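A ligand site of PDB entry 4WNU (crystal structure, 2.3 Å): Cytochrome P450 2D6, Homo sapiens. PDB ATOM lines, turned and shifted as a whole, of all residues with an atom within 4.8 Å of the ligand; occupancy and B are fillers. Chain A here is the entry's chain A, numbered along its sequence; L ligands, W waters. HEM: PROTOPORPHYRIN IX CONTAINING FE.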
ATOM      1  N   LEU A  69      27.810  14.473 -25.165  1.00  0.00           N
ATOM      2  CA  LEU A  69      27.630  13.657 -26.380  1.00  0.00           C
ATOM      3  C   LEU A  69      26.453  14.083 -27.266  1.00  0.00           C
ATOM      4  O   LEU A  69      26.404  13.744 -28.453  1.00  0.00           O
ATOM      5  CB  LEU A  69      27.471  12.172 -26.019  1.00  0.00           C
ATOM      6  CG  LEU A  69      28.629  11.418 -25.330  1.00  0.00           C
ATOM      7  CD1 LEU A  69      28.452   9.894 -25.427  1.00  0.00           C
ATOM      8  CD2 LEU A  69      29.993  11.828 -25.842  1.00  0.00           C
ATOM      9  N   ARG A  79      37.559  10.083 -32.149  1.00  0.00           N
ATOM     10  CA  ARG A  79      38.268   9.105 -31.323  1.00  0.00           C
ATOM     11  C   ARG A  79      39.704   9.566 -31.117  1.00  0.00           C
ATOM     12  O   ARG A  79      40.301  10.180 -31.983  1.00  0.00           O
ATOM     13  CB  ARG A  79      38.265   7.707 -31.979  1.00  0.00           C
ATOM     14  CG  ARG A  79      36.903   7.126 -32.241  1.00  0.00           C
ATOM     15  CD  ARG A  79      36.207   6.684 -30.969  1.00  0.00           C
ATOM     16  NE  ARG A  79      35.045   5.870 -31.266  1.00  0.00           N
ATOM     17  CZ  ARG A  79      33.950   5.831 -30.514  1.00  0.00           C
ATOM     18  NH1 ARG A  79      32.935   5.062 -30.865  1.00  0.00           N
ATOM     19  NH2 ARG A  79      33.871   6.572 -29.410  1.00  0.00           N
ATOM     20  N   VAL A  97      35.141   1.543 -38.655  1.00  0.00           N
ATOM     21  CA  VAL A  97      34.104   2.411 -38.099  1.00  0.00           C
ATOM     22  C   VAL A  97      34.381   2.719 -36.635  1.00  0.00           C
ATOM     23  O   VAL A  97      34.320   3.864 -36.239  1.00  0.00           O
ATOM     24  CB  VAL A  97      32.678   1.784 -38.178  1.00  0.00           C
ATOM     25  CG1 VAL A  97      31.661   2.708 -37.475  1.00  0.00           C
ATOM     26  CG2 VAL A  97      32.247   1.611 -39.575  1.00  0.00           C
ATOM     27  N   PHE A  98      34.691   1.691 -35.850  1.00  0.00           N
ATOM     28  CA  PHE A  98      34.783   1.862 -34.397  1.00  0.00           C
ATOM     29  C   PHE A  98      35.838   2.906 -33.977  1.00  0.00           C
ATOM     30  O   PHE A  98      35.567   3.787 -33.156  1.00  0.00           O
ATOM     31  CB  PHE A  98      35.085   0.497 -33.758  1.00  0.00           C
ATOM     32  CG  PHE A  98      34.927   0.457 -32.282  1.00  0.00           C
ATOM     33  CD1 PHE A  98      33.768  -0.043 -31.711  1.00  0.00           C
ATOM     34  CD2 PHE A  98      35.956   0.884 -31.457  1.00  0.00           C
ATOM     35  CE1 PHE A  98      33.618  -0.096 -30.324  1.00  0.00           C
ATOM     36  CE2 PHE A  98      35.815   0.852 -30.062  1.00  0.00           C
ATOM     37  CZ  PHE A  98      34.647   0.351 -29.500  1.00  0.00           C
ATOM     38  N   TRP A 106      34.839   7.931 -41.503  1.00  0.00           N
ATOM     39  CA  TRP A 106      33.932   7.390 -40.484  1.00  0.00           C
ATOM     40  C   TRP A 106      32.477   7.489 -40.931  1.00  0.00           C
ATOM     41  O   TRP A 106      31.720   6.539 -40.800  1.00  0.00           O
ATOM     42  CB  TRP A 106      34.058   8.118 -39.134  1.00  0.00           C
ATOM     43  CG  TRP A 106      32.910   7.783 -38.218  1.00  0.00           C
ATOM     44  CD1 TRP A 106      32.744   6.632 -37.469  1.00  0.00           C
ATOM     45  CD2 TRP A 106      31.749   8.583 -37.958  1.00  0.00           C
ATOM     46  NE1 TRP A 106      31.565   6.678 -36.779  1.00  0.00           N
ATOM     47  CE2 TRP A 106      30.927   7.861 -37.064  1.00  0.00           C
ATOM     48  CE3 TRP A 106      31.325   9.850 -38.400  1.00  0.00           C
ATOM     49  CZ2 TRP A 106      29.714   8.367 -36.581  1.00  0.00           C
ATOM     50  CZ3 TRP A 106      30.092  10.346 -37.917  1.00  0.00           C
ATOM     51  CH2 TRP A 106      29.312   9.605 -37.012  1.00  0.00           C
ATOM     52  N   ARG A 110      29.853   4.578 -41.229  1.00  0.00           N
ATOM     53  CA  ARG A 110      28.759   4.648 -40.250  1.00  0.00           C
ATOM     54  C   ARG A 110      27.419   4.513 -40.941  1.00  0.00           C
ATOM     55  O   ARG A 110      26.612   3.639 -40.611  1.00  0.00           O
ATOM     56  CB  ARG A 110      28.817   5.973 -39.473  1.00  0.00           C
ATOM     57  CG  ARG A 110      27.645   6.208 -38.529  1.00  0.00           C
ATOM     58  CD  ARG A 110      27.750   5.289 -37.294  1.00  0.00           C
ATOM     59  NE  ARG A 110      26.551   5.389 -36.445  1.00  0.00           N
ATOM     60  CZ  ARG A 110      26.509   5.127 -35.133  1.00  0.00           C
ATOM     61  NH1 ARG A 110      27.599   4.770 -34.458  1.00  0.00           N
ATOM     62  NH2 ARG A 110      25.366   5.242 -34.495  1.00  0.00           N
ATOM     63  N   ILE A 164      26.778 -12.583 -36.223  1.00  0.00           N
ATOM     64  CA  ILE A 164      27.655 -11.692 -36.975  1.00  0.00           C
ATOM     65  C   ILE A 164      28.106 -12.324 -38.299  1.00  0.00           C
ATOM     66  O   ILE A 164      28.206 -11.638 -39.319  1.00  0.00           O
ATOM     67  CB  ILE A 164      28.917 -11.315 -36.172  1.00  0.00           C
ATOM     68  CG1 ILE A 164      28.573 -10.795 -34.765  1.00  0.00           C
ATOM     69  CG2 ILE A 164      29.737 -10.268 -36.959  1.00  0.00           C
ATOM     70  CD1 ILE A 164      27.708  -9.551 -34.758  1.00  0.00           C
ATOM     71  N   LEU A 167      25.236 -11.869 -40.636  1.00  0.00           N
ATOM     72  CA  LEU A 167      25.147 -10.478 -41.090  1.00  0.00           C
ATOM     73  C   LEU A 167      26.243 -10.128 -42.095  1.00  0.00           C
ATOM     74  O   LEU A 167      26.002  -9.384 -43.050  1.00  0.00           O
ATOM     75  CB  LEU A 167      25.231  -9.526 -39.888  1.00  0.00           C
ATOM     76  CG  LEU A 167      25.715  -8.092 -40.133  1.00  0.00           C
ATOM     77  CD1 LEU A 167      24.682  -7.266 -40.927  1.00  0.00           C
ATOM     78  CD2 LEU A 167      26.062  -7.385 -38.806  1.00  0.00           C
ATOM     79  N   LEU A 280      32.901  -5.282 -36.713  1.00  0.00           N
ATOM     80  CA  LEU A 280      31.580  -5.807 -36.358  1.00  0.00           C
ATOM     81  C   LEU A 280      31.692  -7.091 -35.489  1.00  0.00           C
ATOM     82  O   LEU A 280      30.977  -7.224 -34.499  1.00  0.00           O
ATOM     83  CB  LEU A 280      30.724  -6.042 -37.584  1.00  0.00           C
ATOM     84  CG  LEU A 280      30.383  -4.775 -38.368  1.00  0.00           C
ATOM     85  CD1 LEU A 280      29.770  -5.125 -39.734  1.00  0.00           C
ATOM     86  CD2 LEU A 280      29.428  -3.834 -37.577  1.00  0.00           C
ATOM     87  N   ALA A 283      33.438  -5.997 -31.971  1.00  0.00           N
ATOM     88  CA  ALA A 283      32.528  -5.175 -31.165  1.00  0.00           C
ATOM     89  C   ALA A 283      31.247  -5.926 -30.762  1.00  0.00           C
ATOM     90  O   ALA A 283      30.698  -5.679 -29.690  1.00  0.00           O
ATOM     91  CB  ALA A 283      32.158  -3.896 -31.889  1.00  0.00           C
ATOM     92  N   GLY A 284      30.820  -6.869 -31.608  1.00  0.00           N
ATOM     93  CA  GLY A 284      29.540  -7.520 -31.448  1.00  0.00           C
ATOM     94  C   GLY A 284      29.512  -8.877 -30.754  1.00  0.00           C
ATOM     95  O   GLY A 284      28.468  -9.284 -30.268  1.00  0.00           O
ATOM     96  N   THR A 287      30.335  -8.491 -26.360  1.00  0.00           N
ATOM     97  CA  THR A 287      29.293  -7.680 -25.702  1.00  0.00           C
ATOM     98  C   THR A 287      27.977  -8.432 -25.528  1.00  0.00           C
ATOM     99  O   THR A 287      27.456  -8.593 -24.421  1.00  0.00           O
ATOM    100  CB  THR A 287      29.001  -6.381 -26.478  1.00  0.00           C
ATOM    101  OG1 THR A 287      28.805  -6.684 -27.884  1.00  0.00           O
ATOM    102  CG2 THR A 287      30.164  -5.411 -26.308  1.00  0.00           C
ATOM    103  N   THR A 288      27.445  -8.919 -26.640  1.00  0.00           N
ATOM    104  CA  THR A 288      26.163  -9.596 -26.640  1.00  0.00           C
ATOM    105  C   THR A 288      26.275 -10.902 -25.830  1.00  0.00           C
ATOM    106  O   THR A 288      25.385 -11.274 -25.098  1.00  0.00           O
ATOM    107  CB  THR A 288      25.694  -9.862 -28.072  1.00  0.00           C
ATOM    108  OG1 THR A 288      25.858  -8.662 -28.823  1.00  0.00           O
ATOM    109  CG2 THR A 288      24.250 -10.267 -28.099  1.00  0.00           C
ATOM    110  N   THR A 291      26.552 -10.193 -22.039  1.00  0.00           N
ATOM    111  CA  THR A 291      25.202  -9.816 -21.628  1.00  0.00           C
ATOM    112  C   THR A 291      24.318 -11.048 -21.413  1.00  0.00           C
ATOM    113  O   THR A 291      23.653 -11.168 -20.395  1.00  0.00           O
ATOM    114  CB  THR A 291      24.522  -8.903 -22.643  1.00  0.00           C
ATOM    115  OG1 THR A 291      25.288  -7.714 -22.804  1.00  0.00           O
ATOM    116  CG2 THR A 291      23.123  -8.525 -22.171  1.00  0.00           C
ATOM    117  N   GLN A 342      20.906  -5.822 -18.633  1.00  0.00           N
ATOM    118  CA  GLN A 342      21.875  -4.848 -19.170  1.00  0.00           C
ATOM    119  C   GLN A 342      22.218  -3.753 -18.168  1.00  0.00           C
ATOM    120  O   GLN A 342      23.373  -3.307 -18.057  1.00  0.00           O
ATOM    121  CB  GLN A 342      21.350  -4.190 -20.457  1.00  0.00           C
ATOM    122  CG  GLN A 342      21.096  -5.138 -21.636  1.00  0.00           C
ATOM    123  CD  GLN A 342      20.945  -4.333 -22.936  1.00  0.00           C
ATOM    124  OE1 GLN A 342      19.834  -4.068 -23.387  1.00  0.00           O
ATOM    125  NE2 GLN A 342      22.076  -3.894 -23.495  1.00  0.00           N
ATOM    126  N   ILE A 347      28.107  -3.970 -18.539  1.00  0.00           N
ATOM    127  CA  ILE A 347      29.266  -4.652 -19.104  1.00  0.00           C
ATOM    128  C   ILE A 347      30.367  -3.733 -19.631  1.00  0.00           C
ATOM    129  O   ILE A 347      31.525  -4.146 -19.696  1.00  0.00           O
ATOM    130  CB  ILE A 347      28.844  -5.627 -20.249  1.00  0.00           C
ATOM    131  CG1 ILE A 347      28.395  -4.863 -21.502  1.00  0.00           C
ATOM    132  CG2 ILE A 347      27.751  -6.528 -19.793  1.00  0.00           C
ATOM    133  CD1 ILE A 347      28.072  -5.815 -22.710  1.00  0.00           C
ATOM    134  N   VAL A 348      30.016  -2.511 -20.013  1.00  0.00           N
ATOM    135  CA  VAL A 348      31.038  -1.561 -20.450  1.00  0.00           C
ATOM    136  C   VAL A 348      30.950  -0.291 -19.607  1.00  0.00           C
ATOM    137  O   VAL A 348      30.495   0.753 -20.090  1.00  0.00           O
ATOM    138  CB  VAL A 348      30.924  -1.265 -21.981  1.00  0.00           C
ATOM    139  CG1 VAL A 348      31.459  -2.434 -22.785  1.00  0.00           C
ATOM    140  CG2 VAL A 348      29.504  -1.022 -22.394  1.00  0.00           C
ATOM    141  N   GLY A 351      32.405   2.924 -21.032  1.00  0.00           N
ATOM    142  CA  GLY A 351      32.129   3.097 -22.445  1.00  0.00           C
ATOM    143  C   GLY A 351      33.317   2.953 -23.372  1.00  0.00           C
ATOM    144  O   GLY A 351      34.218   2.140 -23.147  1.00  0.00           O
ATOM    145  N   VAL A 352      33.340   3.796 -24.407  1.00  0.00           N
ATOM    146  CA  VAL A 352      34.470   3.880 -25.322  1.00  0.00           C
ATOM    147  C   VAL A 352      34.917   5.321 -25.367  1.00  0.00           C
ATOM    148  O   VAL A 352      34.076   6.223 -25.437  1.00  0.00           O
ATOM    149  CB  VAL A 352      34.081   3.398 -26.747  1.00  0.00           C
ATOM    150  CG1 VAL A 352      35.234   3.600 -27.737  1.00  0.00           C
ATOM    151  CG2 VAL A 352      33.594   1.945 -26.711  1.00  0.00           C
ATOM    152  N   HIS A 354      36.042   9.001 -26.283  1.00  0.00           N
ATOM    153  CA  HIS A 354      35.838  10.004 -27.320  1.00  0.00           C
ATOM    154  C   HIS A 354      36.977  11.008 -27.250  1.00  0.00           C
ATOM    155  O   HIS A 354      37.706  11.068 -26.255  1.00  0.00           O
ATOM    156  CB  HIS A 354      34.509  10.745 -27.114  1.00  0.00           C
ATOM    157  CG  HIS A 354      33.290   9.892 -27.318  1.00  0.00           C
ATOM    158  ND1 HIS A 354      32.306  10.215 -28.223  1.00  0.00           N
ATOM    159  CD2 HIS A 354      32.901   8.736 -26.735  1.00  0.00           C
ATOM    160  CE1 HIS A 354      31.366   9.283 -28.199  1.00  0.00           C
ATOM    161  NE2 HIS A 354      31.703   8.381 -27.289  1.00  0.00           N
ATOM    162  N   LEU A 377      29.513   5.247 -18.007  1.00  0.00           N
ATOM    163  CA  LEU A 377      28.169   4.729 -18.232  1.00  0.00           C
ATOM    164  C   LEU A 377      27.633   4.042 -16.994  1.00  0.00           C
ATOM    165  O   LEU A 377      26.444   4.111 -16.714  1.00  0.00           O
ATOM    166  CB  LEU A 377      28.147   3.751 -19.414  1.00  0.00           C
ATOM    167  CG  LEU A 377      28.514   4.356 -20.776  1.00  0.00           C
ATOM    168  CD1 LEU A 377      28.395   3.314 -21.944  1.00  0.00           C
ATOM    169  CD2 LEU A 377      27.655   5.591 -21.029  1.00  0.00           C
ATOM    170  N   PRO A 413      22.964   1.869 -21.816  1.00  0.00           N
ATOM    171  CA  PRO A 413      24.074   0.901 -21.939  1.00  0.00           C
ATOM    172  C   PRO A 413      24.845   0.974 -23.257  1.00  0.00           C
ATOM    173  O   PRO A 413      25.949   0.429 -23.326  1.00  0.00           O
ATOM    174  CB  PRO A 413      23.363  -0.439 -21.843  1.00  0.00           C
ATOM    175  CG  PRO A 413      22.027  -0.170 -22.459  1.00  0.00           C
ATOM    176  CD  PRO A 413      21.657   1.224 -21.977  1.00  0.00           C
ATOM    177  N   PHE A 414      24.266   1.631 -24.263  1.00  0.00           N
ATOM    178  CA  PHE A 414      24.864   1.777 -25.591  1.00  0.00           C
ATOM    179  C   PHE A 414      25.439   3.174 -25.847  1.00  0.00           C
ATOM    180  O   PHE A 414      25.792   3.506 -26.988  1.00  0.00           O
ATOM    181  CB  PHE A 414      23.813   1.499 -26.662  1.00  0.00           C
ATOM    182  CG  PHE A 414      23.203   0.102 -26.606  1.00  0.00           C
ATOM    183  CD1 PHE A 414      21.898  -0.067 -26.145  1.00  0.00           C
ATOM    184  CD2 PHE A 414      23.902  -1.007 -27.066  1.00  0.00           C
ATOM    185  CE1 PHE A 414      21.313  -1.344 -26.124  1.00  0.00           C
ATOM    186  CE2 PHE A 414      23.326  -2.263 -27.036  1.00  0.00           C
ATOM    187  CZ  PHE A 414      22.042  -2.431 -26.565  1.00  0.00           C
ATOM    188  N   SER A 415      25.475   4.008 -24.800  1.00  0.00           N
ATOM    189  CA  SER A 415      25.933   5.406 -24.893  1.00  0.00           C
ATOM    190  C   SER A 415      24.920   6.254 -25.648  1.00  0.00           C
ATOM    191  O   SER A 415      23.733   5.899 -25.723  1.00  0.00           O
ATOM    192  CB  SER A 415      27.317   5.511 -25.564  1.00  0.00           C
ATOM    193  OG  SER A 415      27.950   6.742 -25.273  1.00  0.00           O
ATOM    194  N   ALA A 416      25.381   7.375 -26.212  1.00  0.00           N
ATOM    195  CA  ALA A 416      24.505   8.397 -26.776  1.00  0.00           C
ATOM    196  C   ALA A 416      25.229   9.208 -27.852  1.00  0.00           C
ATOM    197  O   ALA A 416      26.461   9.180 -27.914  1.00  0.00           O
ATOM    198  CB  ALA A 416      23.987   9.339 -25.652  1.00  0.00           C
ATOM    199  N   ARG A 418      26.161  10.808 -31.836  1.00  0.00           N
ATOM    200  CA  ARG A 418      26.556  10.304 -33.165  1.00  0.00           C
ATOM    201  C   ARG A 418      27.295   8.965 -33.136  1.00  0.00           C
ATOM    202  O   ARG A 418      27.220   8.173 -34.094  1.00  0.00           O
ATOM    203  CB  ARG A 418      27.469  11.307 -33.902  1.00  0.00           C
ATOM    204  CG  ARG A 418      26.795  12.506 -34.517  1.00  0.00           C
ATOM    205  CD  ARG A 418      27.491  13.777 -34.030  1.00  0.00           C
ATOM    206  NE  ARG A 418      27.183  14.965 -34.821  1.00  0.00           N
ATOM    207  CZ  ARG A 418      26.152  15.760 -34.613  1.00  0.00           C
ATOM    208  NH1 ARG A 418      25.971  16.824 -35.382  1.00  0.00           N
ATOM    209  NH2 ARG A 418      25.282  15.498 -33.646  1.00  0.00           N
ATOM    210  N   ARG A 419      28.029   8.708 -32.059  1.00  0.00           N
ATOM    211  CA  ARG A 419      28.863   7.494 -32.016  1.00  0.00           C
ATOM    212  C   ARG A 419      28.258   6.326 -31.218  1.00  0.00           C
ATOM    213  O   ARG A 419      28.867   5.266 -31.088  1.00  0.00           O
ATOM    214  CB  ARG A 419      30.239   7.866 -31.476  1.00  0.00           C
ATOM    215  CG  ARG A 419      31.056   8.622 -32.532  1.00  0.00           C
ATOM    216  CD  ARG A 419      31.752   7.595 -33.465  1.00  0.00           C
ATOM    217  NE  ARG A 419      32.893   8.285 -34.004  1.00  0.00           N
ATOM    218  CZ  ARG A 419      34.008   7.745 -34.474  1.00  0.00           C
ATOM    219  NH1 ARG A 419      34.194   6.418 -34.555  1.00  0.00           N
ATOM    220  NH2 ARG A 419      34.924   8.610 -34.895  1.00  0.00           N
ATOM    221  N   ALA A 420      27.049   6.524 -30.693  1.00  0.00           N
ATOM    222  CA  ALA A 420      26.328   5.468 -29.988  1.00  0.00           C
ATOM    223  C   ALA A 420      26.329   4.136 -30.766  1.00  0.00           C
ATOM    224  O   ALA A 420      26.284   4.136 -32.016  1.00  0.00           O
ATOM    225  CB  ALA A 420      24.882   5.915 -29.728  1.00  0.00           C
ATOM    226  N   CYS A 421      26.402   3.015 -30.033  1.00  0.00           N
ATOM    227  CA  CYS A 421      26.458   1.673 -30.622  1.00  0.00           C
ATOM    228  C   CYS A 421      25.558   1.536 -31.851  1.00  0.00           C
ATOM    229  O   CYS A 421      24.354   1.658 -31.743  1.00  0.00           O
ATOM    230  CB  CYS A 421      26.034   0.612 -29.591  1.00  0.00           C
ATOM    231  SG  CYS A 421      26.156  -1.109 -30.196  1.00  0.00           S
ATOM    232  N   LEU A 422      26.166   1.287 -33.013  1.00  0.00           N
ATOM    233  CA  LEU A 422      25.350   1.065 -34.221  1.00  0.00           C
ATOM    234  C   LEU A 422      24.791  -0.352 -34.225  1.00  0.00           C
ATOM    235  O   LEU A 422      23.928  -0.681 -35.016  1.00  0.00           O
ATOM    236  CB  LEU A 422      26.165   1.322 -35.497  1.00  0.00           C
ATOM    237  CG  LEU A 422      27.424   0.513 -35.829  1.00  0.00           C
ATOM    238  CD1 LEU A 422      27.114  -0.904 -36.368  1.00  0.00           C
ATOM    239  CD2 LEU A 422      28.200   1.287 -36.885  1.00  0.00           C
ATOM    240  N   GLY A 423      25.295  -1.187 -33.330  1.00  0.00           N
ATOM    241  CA  GLY A 423      24.795  -2.547 -33.227  1.00  0.00           C
ATOM    242  C   GLY A 423      23.494  -2.645 -32.449  1.00  0.00           C
ATOM    243  O   GLY A 423      22.889  -3.701 -32.406  1.00  0.00           O
ATOM    244  N   LEU A 426      20.435  -4.685 -33.583  1.00  0.00           N
ATOM    245  CA  LEU A 426      20.704  -6.111 -33.702  1.00  0.00           C
ATOM    246  C   LEU A 426      20.850  -6.762 -32.328  1.00  0.00           C
ATOM    247  O   LEU A 426      20.352  -7.866 -32.075  1.00  0.00           O
ATOM    248  CB  LEU A 426      21.959  -6.348 -34.527  1.00  0.00           C
ATOM    249  CG  LEU A 426      22.418  -7.798 -34.729  1.00  0.00           C
ATOM    250  CD1 LEU A 426      21.303  -8.679 -35.274  1.00  0.00           C
ATOM    251  CD2 LEU A 426      23.662  -7.828 -35.631  1.00  0.00           C
ATOM    252  N   ALA A 427      21.539  -6.066 -31.427  1.00  0.00           N
ATOM    253  CA  ALA A 427      21.747  -6.546 -30.081  1.00  0.00           C
ATOM    254  C   ALA A 427      20.399  -6.759 -29.387  1.00  0.00           C
ATOM    255  O   ALA A 427      20.206  -7.772 -28.693  1.00  0.00           O
ATOM    256  CB  ALA A 427      22.612  -5.577 -29.294  1.00  0.00           C
ATOM    257  N   GLU A 430      18.905  -9.890 -30.687  1.00  0.00           N
ATOM    258  CA  GLU A 430      19.596 -11.041 -30.145  1.00  0.00           C
ATOM    259  C   GLU A 430      19.258 -11.329 -28.676  1.00  0.00           C
ATOM    260  O   GLU A 430      19.005 -12.488 -28.305  1.00  0.00           O
ATOM    261  CB  GLU A 430      21.118 -10.869 -30.290  1.00  0.00           C
ATOM    262  CG  GLU A 430      21.650 -11.090 -31.692  1.00  0.00           C
ATOM    263  CD  GLU A 430      23.160 -11.065 -31.721  1.00  0.00           C
ATOM    264  OE1 GLU A 430      23.781 -12.087 -31.372  1.00  0.00           O
ATOM    265  OE2 GLU A 430      23.748 -10.010 -32.044  1.00  0.00           O
ATOM    266  N   LEU A 431      19.270 -10.285 -27.846  1.00  0.00           N
ATOM    267  CA  LEU A 431      18.947 -10.475 -26.421  1.00  0.00           C
ATOM    268  C   LEU A 431      17.540 -11.013 -26.304  1.00  0.00           C
ATOM    269  O   LEU A 431      17.317 -11.997 -25.600  1.00  0.00           O
ATOM    270  CB  LEU A 431      19.087  -9.176 -25.634  1.00  0.00           C
ATOM    271  CG  LEU A 431      20.483  -8.573 -25.604  1.00  0.00           C
ATOM    272  CD1 LEU A 431      20.558  -7.311 -24.664  1.00  0.00           C
ATOM    273  CD2 LEU A 431      21.477  -9.627 -25.220  1.00  0.00           C
HETATM  274  CHA HEM L   1      29.993   1.207 -30.078  1.00  0.00           C
HETATM  275  CHB HEM L   1      27.927  -1.123 -26.325  1.00  0.00           C
HETATM  276  CHC HEM L   1      26.653  -4.778 -29.280  1.00  0.00           C
HETATM  277  CHD HEM L   1      29.017  -2.581 -32.924  1.00  0.00           C
HETATM  278  C1A HEM L   1      29.562   0.897 -28.807  1.00  0.00           C
HETATM  279  C2A HEM L   1      29.679   1.748 -27.641  1.00  0.00           C
HETATM  280  C3A HEM L   1      29.117   1.112 -26.605  1.00  0.00           C
HETATM  281  C4A HEM L   1      28.581  -0.161 -27.075  1.00  0.00           C
HETATM  282  CMA HEM L   1      29.033   1.624 -25.192  1.00  0.00           C
HETATM  283  CAA HEM L   1      30.382   3.112 -27.618  1.00  0.00           C
HETATM  284  CBA HEM L   1      29.521   4.288 -28.089  1.00  0.00           C
HETATM  285  CGA HEM L   1      30.401   5.524 -27.963  1.00  0.00           C
HETATM  286  O1A HEM L   1      31.456   5.583 -28.656  1.00  0.00           O
HETATM  287  O2A HEM L   1      30.068   6.432 -27.142  1.00  0.00           O
HETATM  288  C1B HEM L   1      27.379  -2.326 -26.778  1.00  0.00           C
HETATM  289  C2B HEM L   1      26.574  -3.274 -26.015  1.00  0.00           C
HETATM  290  C3B HEM L   1      26.231  -4.292 -26.839  1.00  0.00           C
HETATM  291  C4B HEM L   1      26.793  -4.007 -28.142  1.00  0.00           C
HETATM  292  CMB HEM L   1      26.235  -3.092 -24.555  1.00  0.00           C
HETATM  293  CAB HEM L   1      25.400  -5.571 -26.584  1.00  0.00           C
HETATM  294  CBB HEM L   1      24.589  -5.777 -25.549  1.00  0.00           C
HETATM  295  C1C HEM L   1      27.135  -4.475 -30.542  1.00  0.00           C
HETATM  296  C2C HEM L   1      26.893  -5.234 -31.759  1.00  0.00           C
HETATM  297  C3C HEM L   1      27.587  -4.630 -32.747  1.00  0.00           C
HETATM  298  C4C HEM L   1      28.229  -3.460 -32.204  1.00  0.00           C
HETATM  299  CMC HEM L   1      26.044  -6.496 -31.834  1.00  0.00           C
HETATM  300  CAC HEM L   1      27.701  -4.954 -34.258  1.00  0.00           C
HETATM  301  CBC HEM L   1      26.718  -5.475 -34.970  1.00  0.00           C
HETATM  302  C1D HEM L   1      29.504  -1.372 -32.510  1.00  0.00           C
HETATM  303  C2D HEM L   1      30.268  -0.406 -33.273  1.00  0.00           C
HETATM  304  C3D HEM L   1      30.540   0.638 -32.488  1.00  0.00           C
HETATM  305  C4D HEM L   1      29.946   0.391 -31.196  1.00  0.00           C
HETATM  306  CMD HEM L   1      30.687  -0.584 -34.725  1.00  0.00           C
HETATM  307  CAD HEM L   1      31.308   1.918 -32.873  1.00  0.00           C
HETATM  308  CBD HEM L   1      30.264   2.937 -33.324  1.00  0.00           C
HETATM  309  CGD HEM L   1      30.930   4.165 -33.925  1.00  0.00           C
HETATM  310  O1D HEM L   1      30.292   4.867 -34.742  1.00  0.00           O
HETATM  311  O2D HEM L   1      32.114   4.459 -33.629  1.00  0.00           O
HETATM  312  NA  HEM L   1      28.878  -0.241 -28.429  1.00  0.00           N
HETATM  313  NB  HEM L   1      27.495  -2.830 -28.041  1.00  0.00           N
HETATM  314  NC  HEM L   1      27.944  -3.421 -30.869  1.00  0.00           N
HETATM  315  ND  HEM L   1      29.336  -0.830 -31.257  1.00  0.00           N
HETATM  316 FE   HEM L   1      28.235  -1.742 -29.739  1.00  0.00          FE
HETATM  317  O   HOH W   1      31.019   5.365 -24.455  1.00  0.00           O
HETATM  318  O   HOH W   2      24.250  -5.183 -22.223  1.00  0.00           O
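An iron atom (FE) of the ligand is bound by the side-chain sulfur of Cys 421 (2.2 Å). NE2 of His 354 sits at hydrogen-bond distance from O2A of the ligand (2.5 Å). An oxygen (O1A) of the ligand lies within salt-bridge range of the guanidinium group (NH1) of Arg 79, 2.7 Å away. The guanidinium group (NH1) of Arg 110 is in salt-bridge range of an oxygen (O1D) of the ligand (2.7 Å). The side-chain hydroxyl (OG) of Ser 415 is in hydrogen-bond range of an oxygen (O2A) of the ligand (2.8 Å). An oxygen (O2D) of the ligand is in salt-bridge range of the guanidinium group of Arg 419 (3.0 Å). The indole nitrogen (NE1) of Trp 106 is in hydrogen-bond range of an oxygen (O1D) of the ligand.
N of Gly 423 lies close to SG of Cys 421, at 3.3 Å. O of Phe 414 sits at hydrogen-bond distance from N of Cys 421. O of Phe 98 sits at hydrogen-bond distance from NE of Arg 79 (2.9 Å). NH1 of Arg 110 sits close to O of Arg 418, at 3.4 Å. The backbone carbonyl oxygen (O) of Phe 98 lies within hydrogen-bond range of the guanidinium group (NH1) of Arg 419, 3.3 Å away. The backbone carbonyl oxygen of Val 97 is in hydrogen-bond range of the guanidinium group of Arg 419. O of Thr 287 lies within hydrogen-bond range of OG1 of Thr 291. The backbone carbonyl oxygen (O) of Gly 284 lies within hydrogen-bond range of the side-chain hydroxyl (OG1) of Thr 288 (3.0 Å).
The backbone carbonyl oxygen (O) of Val 97 lies close to an oxygen (O2D) of the ligand. Residues that only touch the ligand: Thr 287, Phe 98, Thr 291, Gly 284, Gly 423, Val 352, Phe 414, Ala 283, Leu 422, Thr 288, Leu 377, Pro 413, Gln 342, Ile 347, Val 348, Ala 427, Ala 420, Leu 280 and Leu 426. The nearest printed residue that does not touch the ligand is Leu 69 (4.2 Å).
Water W1 lies within hydrogen-bond range of N of Val 352 (2.8 Å), O2A of the ligand (3.0 Å) and OG of Ser 415 (3.5 Å). Water W2 lies within hydrogen-bond range of OG1 of Thr 291 (2.8 Å) and NE2 of Gln 342 (2.8 Å).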
